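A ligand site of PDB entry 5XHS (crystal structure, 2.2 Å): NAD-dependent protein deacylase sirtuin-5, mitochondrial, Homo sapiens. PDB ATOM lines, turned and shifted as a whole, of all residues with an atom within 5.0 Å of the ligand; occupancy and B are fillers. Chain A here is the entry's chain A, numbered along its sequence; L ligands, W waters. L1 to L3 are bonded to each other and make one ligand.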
ATOM      1  N   ARG A  57     -21.647  16.616 -17.218  1.00  0.00           N
ATOM      2  CA  ARG A  57     -22.689  15.643 -16.889  1.00  0.00           C
ATOM      3  C   ARG A  57     -22.379  14.884 -15.604  1.00  0.00           C
ATOM      4  O   ARG A  57     -23.251  14.788 -14.720  1.00  0.00           O
ATOM      5  CB  ARG A  57     -22.857  14.637 -18.051  1.00  0.00           C
ATOM      6  CG  ARG A  57     -23.464  15.194 -19.345  1.00  0.00           C
ATOM      7  CD  ARG A  57     -24.940  15.571 -19.183  1.00  0.00           C
ATOM      8  NE  ARG A  57     -25.748  14.448 -18.690  1.00  0.00           N
ATOM      9  CZ  ARG A  57     -26.209  13.456 -19.452  1.00  0.00           C
ATOM     10  NH1 ARG A  57     -25.951  13.427 -20.756  1.00  0.00           N
ATOM     11  NH2 ARG A  57     -26.934  12.477 -18.912  1.00  0.00           N
ATOM     12  N   ALA A  68     -25.065  20.256 -17.201  1.00  0.00           N
ATOM     13  CA  ALA A  68     -25.753  20.301 -18.482  1.00  0.00           C
ATOM     14  C   ALA A  68     -27.265  20.235 -18.292  1.00  0.00           C
ATOM     15  O   ALA A  68     -28.003  20.993 -18.932  1.00  0.00           O
ATOM     16  CB  ALA A  68     -25.261  19.158 -19.364  1.00  0.00           C
ATOM     17  N   ALA A  72     -28.983  22.860 -20.587  1.00  0.00           N
ATOM     18  CA  ALA A  72     -29.427  22.247 -21.843  1.00  0.00           C
ATOM     19  C   ALA A  72     -30.934  21.972 -21.816  1.00  0.00           C
ATOM     20  O   ALA A  72     -31.379  20.837 -21.940  1.00  0.00           O
ATOM     21  CB  ALA A  72     -28.659  20.952 -22.108  1.00  0.00           C
ATOM     22  N   PHE A  87     -22.519  29.267 -22.005  1.00  0.00           N
ATOM     23  CA  PHE A  87     -22.201  27.859 -21.814  1.00  0.00           C
ATOM     24  C   PHE A  87     -21.765  27.198 -23.121  1.00  0.00           C
ATOM     25  O   PHE A  87     -20.697  26.565 -23.191  1.00  0.00           O
ATOM     26  CB  PHE A  87     -23.441  27.177 -21.225  1.00  0.00           C
ATOM     27  CG  PHE A  87     -23.296  25.705 -20.986  1.00  0.00           C
ATOM     28  CD1 PHE A  87     -22.168  25.200 -20.366  1.00  0.00           C
ATOM     29  CD2 PHE A  87     -24.302  24.823 -21.365  1.00  0.00           C
ATOM     30  CE1 PHE A  87     -22.044  23.844 -20.118  1.00  0.00           C
ATOM     31  CE2 PHE A  87     -24.188  23.463 -21.113  1.00  0.00           C
ATOM     32  CZ  PHE A  87     -23.053  22.980 -20.483  1.00  0.00           C
ATOM     33  N   TYR A  88     -22.574  27.354 -24.170  1.00  0.00           N
ATOM     34  CA  TYR A  88     -22.268  26.726 -25.454  1.00  0.00           C
ATOM     35  C   TYR A  88     -21.138  27.439 -26.216  1.00  0.00           C
ATOM     36  O   TYR A  88     -20.399  26.793 -26.954  1.00  0.00           O
ATOM     37  CB  TYR A  88     -23.561  26.662 -26.293  1.00  0.00           C
ATOM     38  CG  TYR A  88     -24.448  25.516 -25.857  1.00  0.00           C
ATOM     39  CD1 TYR A  88     -25.564  25.732 -25.039  1.00  0.00           C
ATOM     40  CD2 TYR A  88     -24.154  24.197 -26.226  1.00  0.00           C
ATOM     41  CE1 TYR A  88     -26.361  24.656 -24.620  1.00  0.00           C
ATOM     42  CE2 TYR A  88     -24.932  23.133 -25.804  1.00  0.00           C
ATOM     43  CZ  TYR A  88     -26.042  23.364 -25.018  1.00  0.00           C
ATOM     44  OH  TYR A  88     -26.844  22.291 -24.611  1.00  0.00           O
ATOM     45  N   ARG A  91     -18.104  25.872 -24.816  1.00  0.00           N
ATOM     46  CA  ARG A  91     -17.858  24.529 -25.314  1.00  0.00           C
ATOM     47  C   ARG A  91     -17.344  24.535 -26.753  1.00  0.00           C
ATOM     48  O   ARG A  91     -16.503  23.702 -27.106  1.00  0.00           O
ATOM     49  CB  ARG A  91     -19.125  23.693 -25.131  1.00  0.00           C
ATOM     50  CG  ARG A  91     -19.475  23.531 -23.642  1.00  0.00           C
ATOM     51  CD  ARG A  91     -20.797  22.826 -23.430  1.00  0.00           C
ATOM     52  NE  ARG A  91     -20.775  21.457 -23.918  1.00  0.00           N
ATOM     53  CZ  ARG A  91     -21.846  20.659 -23.874  1.00  0.00           C
ATOM     54  NH1 ARG A  91     -22.990  21.110 -23.374  1.00  0.00           N
ATOM     55  NH2 ARG A  91     -21.779  19.430 -24.329  1.00  0.00           N
ATOM     56  N   ILE A 128     -21.576  15.766 -29.373  1.00  0.00           N
ATOM     57  CA  ILE A 128     -21.926  16.964 -30.111  1.00  0.00           C
ATOM     58  C   ILE A 128     -20.690  17.772 -30.504  1.00  0.00           C
ATOM     59  O   ILE A 128     -20.816  18.861 -31.031  1.00  0.00           O
ATOM     60  CB  ILE A 128     -22.948  17.841 -29.355  1.00  0.00           C
ATOM     61  CG1 ILE A 128     -22.357  18.407 -28.060  1.00  0.00           C
ATOM     62  CG2 ILE A 128     -24.264  17.057 -28.999  1.00  0.00           C
ATOM     63  CD1 ILE A 128     -23.073  19.614 -27.594  1.00  0.00           C
ATOM     64  N   HIS A 144     -27.730  13.988 -31.252  1.00  0.00           N
ATOM     65  CA  HIS A 144     -27.983  15.149 -30.413  1.00  0.00           C
ATOM     66  C   HIS A 144     -27.611  16.466 -31.099  1.00  0.00           C
ATOM     67  O   HIS A 144     -27.670  17.513 -30.455  1.00  0.00           O
ATOM     68  CB  HIS A 144     -27.223  15.011 -29.104  1.00  0.00           C
ATOM     69  CG  HIS A 144     -27.830  13.983 -28.198  1.00  0.00           C
ATOM     70  ND1 HIS A 144     -27.204  13.506 -27.076  1.00  0.00           N
ATOM     71  CD2 HIS A 144     -29.005  13.325 -28.285  1.00  0.00           C
ATOM     72  CE1 HIS A 144     -27.967  12.597 -26.500  1.00  0.00           C
ATOM     73  NE2 HIS A 144     -29.074  12.476 -27.207  1.00  0.00           N
ATOM     74  N   VAL A 206     -28.775  21.620 -30.980  1.00  0.00           N
ATOM     75  CA  VAL A 206     -28.508  20.451 -30.154  1.00  0.00           C
ATOM     76  C   VAL A 206     -29.816  20.022 -29.498  1.00  0.00           C
ATOM     77  O   VAL A 206     -30.693  20.830 -29.207  1.00  0.00           O
ATOM     78  CB  VAL A 206     -27.394  20.721 -29.104  1.00  0.00           C
ATOM     79  CG1 VAL A 206     -26.142  21.389 -29.767  1.00  0.00           C
ATOM     80  CG2 VAL A 206     -27.883  21.606 -28.002  1.00  0.00           C
ATOM     81  N   VAL A 207     -29.943  18.734 -29.298  1.00  0.00           N
ATOM     82  CA  VAL A 207     -31.102  18.197 -28.604  1.00  0.00           C
ATOM     83  C   VAL A 207     -30.940  18.503 -27.120  1.00  0.00           C
ATOM     84  O   VAL A 207     -29.938  18.113 -26.498  1.00  0.00           O
ATOM     85  CB  VAL A 207     -31.283  16.691 -28.863  1.00  0.00           C
ATOM     86  CG1 VAL A 207     -32.465  16.160 -28.101  1.00  0.00           C
ATOM     87  CG2 VAL A 207     -31.506  16.421 -30.382  1.00  0.00           C
ATOM     88  N   TRP A 208     -31.901  19.204 -26.552  1.00  0.00           N
ATOM     89  CA  TRP A 208     -31.837  19.499 -25.128  1.00  0.00           C
ATOM     90  C   TRP A 208     -32.567  18.424 -24.305  1.00  0.00           C
ATOM     91  O   TRP A 208     -33.311  17.577 -24.831  1.00  0.00           O
ATOM     92  CB  TRP A 208     -32.408  20.871 -24.864  1.00  0.00           C
ATOM     93  CG  TRP A 208     -31.427  21.947 -25.217  1.00  0.00           C
ATOM     94  CD1 TRP A 208     -30.065  21.851 -25.218  1.00  0.00           C
ATOM     95  CD2 TRP A 208     -31.728  23.288 -25.627  1.00  0.00           C
ATOM     96  NE1 TRP A 208     -29.503  23.036 -25.594  1.00  0.00           N
ATOM     97  CE2 TRP A 208     -30.501  23.933 -25.850  1.00  0.00           C
ATOM     98  CE3 TRP A 208     -32.918  23.996 -25.810  1.00  0.00           C
ATOM     99  CZ2 TRP A 208     -30.435  25.281 -26.246  1.00  0.00           C
ATOM    100  CZ3 TRP A 208     -32.844  25.323 -26.207  1.00  0.00           C
ATOM    101  CH2 TRP A 208     -31.608  25.947 -26.432  1.00  0.00           C
ATOM    102  N   PHE A 209     -32.289  18.450 -23.006  1.00  0.00           N
ATOM    103  CA  PHE A 209     -33.056  17.637 -22.080  1.00  0.00           C
ATOM    104  C   PHE A 209     -34.536  17.966 -22.235  1.00  0.00           C
ATOM    105  O   PHE A 209     -34.914  19.139 -22.291  1.00  0.00           O
ATOM    106  CB  PHE A 209     -32.604  17.871 -20.631  1.00  0.00           C
ATOM    107  CG  PHE A 209     -31.261  17.241 -20.283  1.00  0.00           C
ATOM    108  CD1 PHE A 209     -31.186  15.946 -19.786  1.00  0.00           C
ATOM    109  CD2 PHE A 209     -30.075  17.971 -20.431  1.00  0.00           C
ATOM    110  CE1 PHE A 209     -29.960  15.387 -19.460  1.00  0.00           C
ATOM    111  CE2 PHE A 209     -28.844  17.404 -20.101  1.00  0.00           C
ATOM    112  CZ  PHE A 209     -28.797  16.118 -19.605  1.00  0.00           C
ATOM    113  N   GLY A 210     -35.354  16.919 -22.345  1.00  0.00           N
ATOM    114  CA  GLY A 210     -36.775  17.092 -22.480  1.00  0.00           C
ATOM    115  C   GLY A 210     -37.226  17.342 -23.882  1.00  0.00           C
ATOM    116  O   GLY A 210     -38.339  17.802 -24.102  1.00  0.00           O
ATOM    117  N   GLU A 211     -36.391  17.046 -24.870  1.00  0.00           N
ATOM    118  CA  GLU A 211     -36.715  17.343 -26.246  1.00  0.00           C
ATOM    119  C   GLU A 211     -36.717  16.068 -27.067  1.00  0.00           C
ATOM    120  O   GLU A 211     -36.033  15.087 -26.734  1.00  0.00           O
ATOM    121  CB  GLU A 211     -35.731  18.354 -26.852  1.00  0.00           C
ATOM    122  CG  GLU A 211     -36.190  19.795 -26.766  1.00  0.00           C
ATOM    123  CD  GLU A 211     -35.206  20.790 -27.328  1.00  0.00           C
ATOM    124  OE1 GLU A 211     -34.082  20.398 -27.754  1.00  0.00           O
ATOM    125  OE2 GLU A 211     -35.547  21.990 -27.346  1.00  0.00           O
ATOM    126  N   ASN A 212     -37.479  16.133 -28.154  1.00  0.00           N
ATOM    127  CA  ASN A 212     -37.552  15.072 -29.150  1.00  0.00           C
ATOM    128  C   ASN A 212     -36.271  14.992 -29.985  1.00  0.00           C
ATOM    129  O   ASN A 212     -35.736  16.021 -30.422  1.00  0.00           O
ATOM    130  CB  ASN A 212     -38.775  15.322 -30.066  1.00  0.00           C
ATOM    131  CG  ASN A 212     -39.164  14.099 -30.827  1.00  0.00           C
ATOM    132  OD1 ASN A 212     -38.687  13.007 -30.531  1.00  0.00           O
ATOM    133  ND2 ASN A 212     -40.059  14.251 -31.804  1.00  0.00           N
ATOM    134  N   LEU A 213     -35.785  13.770 -30.250  1.00  0.00           N
ATOM    135  CA  LEU A 213     -34.858  13.557 -31.363  1.00  0.00           C
ATOM    136  C   LEU A 213     -35.510  13.882 -32.698  1.00  0.00           C
ATOM    137  O   LEU A 213     -36.708  13.684 -32.893  1.00  0.00           O
ATOM    138  CB  LEU A 213     -34.395  12.130 -31.423  1.00  0.00           C
ATOM    139  CG  LEU A 213     -33.269  11.675 -30.531  1.00  0.00           C
ATOM    140  CD1 LEU A 213     -33.177  12.511 -29.267  1.00  0.00           C
ATOM    141  CD2 LEU A 213     -33.512  10.231 -30.230  1.00  0.00           C
ATOM    142  N   LEU A 218     -33.866   9.626 -36.545  1.00  0.00           N
ATOM    143  CA  LEU A 218     -34.328   8.359 -35.989  1.00  0.00           C
ATOM    144  C   LEU A 218     -34.636   7.366 -37.081  1.00  0.00           C
ATOM    145  O   LEU A 218     -34.310   6.178 -36.964  1.00  0.00           O
ATOM    146  CB  LEU A 218     -35.565   8.574 -35.130  1.00  0.00           C
ATOM    147  CG  LEU A 218     -35.421   8.853 -33.628  1.00  0.00           C
ATOM    148  CD1 LEU A 218     -36.774   9.183 -33.022  1.00  0.00           C
ATOM    149  CD2 LEU A 218     -34.798   7.665 -32.911  1.00  0.00           C
ATOM    150  N   TYR A 241     -29.404   4.776 -21.911  1.00  0.00           N
ATOM    151  CA  TYR A 241     -29.594   5.718 -23.002  1.00  0.00           C
ATOM    152  C   TYR A 241     -28.230   6.232 -23.437  1.00  0.00           C
ATOM    153  O   TYR A 241     -27.430   6.610 -22.596  1.00  0.00           O
ATOM    154  CB  TYR A 241     -30.484   6.884 -22.593  1.00  0.00           C
ATOM    155  CG  TYR A 241     -30.674   7.867 -23.730  1.00  0.00           C
ATOM    156  CD1 TYR A 241     -31.609   7.625 -24.728  1.00  0.00           C
ATOM    157  CD2 TYR A 241     -29.875   8.988 -23.841  1.00  0.00           C
ATOM    158  CE1 TYR A 241     -31.753   8.462 -25.781  1.00  0.00           C
ATOM    159  CE2 TYR A 241     -30.023   9.857 -24.899  1.00  0.00           C
ATOM    160  CZ  TYR A 241     -30.969   9.584 -25.868  1.00  0.00           C
ATOM    161  OH  TYR A 241     -31.146  10.433 -26.934  1.00  0.00           O
ATOM    162  N   MET A 245     -31.453   2.062 -26.708  1.00  0.00           N
ATOM    163  CA  MET A 245     -32.509   2.239 -27.723  1.00  0.00           C
ATOM    164  C   MET A 245     -32.220   1.455 -28.977  1.00  0.00           C
ATOM    165  O   MET A 245     -33.122   1.267 -29.792  1.00  0.00           O
ATOM    166  CB  MET A 245     -32.657   3.700 -28.173  1.00  0.00           C
ATOM    167  CG  MET A 245     -32.964   4.746 -27.139  1.00  0.00           C
ATOM    168  SD  MET A 245     -34.329   4.306 -26.056  1.00  0.00           S
ATOM    169  CE  MET A 245     -33.533   3.349 -24.789  1.00  0.00           C
ATOM    170  N   PHE A 246     -30.965   1.057 -29.177  1.00  0.00           N
ATOM    171  CA  PHE A 246     -30.477   0.596 -30.462  1.00  0.00           C
ATOM    172  C   PHE A 246     -29.962  -0.840 -30.420  1.00  0.00           C
ATOM    173  O   PHE A 246     -30.379  -1.657 -31.237  1.00  0.00           O
ATOM    174  CB  PHE A 246     -29.364   1.540 -30.946  1.00  0.00           C
ATOM    175  CG  PHE A 246     -29.762   2.993 -30.991  1.00  0.00           C
ATOM    176  CD1 PHE A 246     -31.073   3.373 -31.220  1.00  0.00           C
ATOM    177  CD2 PHE A 246     -28.812   3.969 -30.850  1.00  0.00           C
ATOM    178  CE1 PHE A 246     -31.416   4.699 -31.260  1.00  0.00           C
ATOM    179  CE2 PHE A 246     -29.165   5.306 -30.906  1.00  0.00           C
ATOM    180  CZ  PHE A 246     -30.446   5.671 -31.097  1.00  0.00           C
HETATM  181  C1  LIG L   1     -34.067  13.484 -21.212  1.00  0.00           C
HETATM  182  O1  LIG L   1     -35.027  14.116 -21.444  1.00  0.00           O
HETATM  183  O2  LIG L   1     -33.605  13.508 -19.880  1.00  0.00           O
HETATM  184  C2  LIG L   1     -33.181  12.310 -19.313  1.00  0.00           C
HETATM  185  C3  LIG L   1     -34.315  11.652 -18.534  1.00  0.00           C
HETATM  186  C4  LIG L   1     -34.702  12.100 -17.268  1.00  0.00           C
HETATM  187  C5  LIG L   1     -35.733  11.473 -16.578  1.00  0.00           C
HETATM  188  C6  LIG L   1     -36.377  10.403 -17.145  1.00  0.00           C
HETATM  189  C7  LIG L   1     -35.991   9.956 -18.412  1.00  0.00           C
HETATM  190  C8  LIG L   1     -34.968  10.579 -19.099  1.00  0.00           C
HETATM  191  C1  LG2 L   2     -34.166  12.079 -24.620  1.00  0.00           C
HETATM  192  N1  LG2 L   2     -33.435  12.782 -22.341  1.00  0.00           N
HETATM  193  O1  LG2 L   2     -33.800  10.979 -24.418  1.00  0.00           O
HETATM  194  C2  LG2 L   2     -33.818  13.242 -23.694  1.00  0.00           C
HETATM  195  C3  LG2 L   2     -32.741  14.078 -24.367  1.00  0.00           C
HETATM  196  C4  LG2 L   2     -30.239  14.378 -24.455  1.00  0.00           C
HETATM  197  C5  LG2 L   2     -29.647  15.240 -23.354  1.00  0.00           C
HETATM  198  C6  LG2 L   2     -31.388  13.560 -23.897  1.00  0.00           C
HETATM  199  C7  LG2 L   2     -27.141  17.644 -25.008  1.00  0.00           C
HETATM  200  C8  LG2 L   2     -26.522  18.329 -23.815  1.00  0.00           C
HETATM  201  C9  LG2 L   2     -25.258  19.012 -24.270  1.00  0.00           C
HETATM  202  C10 LG2 L   2     -27.742  16.419 -24.374  1.00  0.00           C
HETATM  203  O2  LG2 L   2     -27.079  15.476 -24.150  1.00  0.00           O
HETATM  204  N2  LG2 L   2     -29.114  16.439 -23.987  1.00  0.00           N
HETATM  205  O3  LG2 L   2     -24.198  18.346 -24.400  1.00  0.00           O
HETATM  206  O4  LG2 L   2     -25.349  20.241 -24.511  1.00  0.00           O
HETATM  207  N1  LG3 L   3     -34.990  12.450 -25.749  1.00  0.00           N
HETATM  208  C1  LG3 L   3     -35.501  11.530 -26.725  1.00  0.00           C
HETATM  209  C2  LG3 L   3     -35.106  10.216 -26.779  1.00  0.00           C
HETATM  210  C3  LG3 L   3     -35.684   9.369 -27.729  1.00  0.00           C
HETATM  211  C4  LG3 L   3     -35.453   7.434 -29.004  1.00  0.00           C
HETATM  212  C5  LG3 L   3     -36.593   7.773 -29.751  1.00  0.00           C
HETATM  213  C6  LG3 L   3     -37.224   9.024 -29.539  1.00  0.00           C
HETATM  214  C7  LG3 L   3     -36.642   9.863 -28.585  1.00  0.00           C
HETATM  215  C8  LG3 L   3     -37.062  11.170 -28.513  1.00  0.00           C
HETATM  216  C9  LG3 L   3     -36.495  11.985 -27.567  1.00  0.00           C
HETATM  217  C10 LG3 L   3     -38.494   9.517 -30.248  1.00  0.00           C
HETATM  218  O1  LG3 L   3     -35.275   8.068 -27.826  1.00  0.00           O
HETATM  219  O2  LG3 L   3     -34.643   6.637 -29.373  1.00  0.00           O
HETATM  220  O   HOH W   1     -23.981  16.560 -21.801  1.00  0.00           O
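O4 of LG2 L2 is in hydrogen-bond range of OH of Tyr 88, 2.5 Å away. O1 of LIG L1 is in hydrogen-bond range of N of Gly 210. The guanidinium group of Arg 91 lies within salt-bridge range of an oxygen (O3) of LG2 L2, 2.7 Å away. The backbone carbonyl oxygen (O) of Val 207 is in hydrogen-bond range of a nitrogen (N2) of LG2 L2, at 3.1 Å. The backbone carbonyl oxygen of Glu 211 is in hydrogen-bond range of a nitrogen (N1) of LG3 L3 (3.0 Å).
The indole nitrogen (NE1) of Trp 208 lies within hydrogen-bond range of the side-chain hydroxyl (OH) of Tyr 88. The backbone NH of Phe 209 is in hydrogen-bond range of the backbone carbonyl oxygen of Ala 72, at 2.8 Å. The side-chain hydroxyl (OH) of Tyr 241 sits at hydrogen-bond distance from a ring nitrogen (NE2) of His 144 (2.9 Å). OE1 of Glu 211 is in hydrogen-bond range of N of Trp 208 (2.8 Å). The backbone NH of Val 207 is in hydrogen-bond range of the backbone carbonyl oxygen of His 144, at 2.8 Å.
Residues that only touch the ligand: Ala 72, Ile 128, His 144, Trp 208, Phe 209, Asn 212, Leu 213, Leu 218, Tyr 241 and Met 245. Hydrophobic or aromatic side chains that line the ligand: Ala 72, Tyr 88, Ile 128, His 144, Phe 209, Leu 213, Leu 218, Tyr 241 and Met 245. Of the 20 residues printed, 15 come within 4 Å of the ligand. Along chain A the residues within 4 Å of the ligand span positions 72 to 245.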
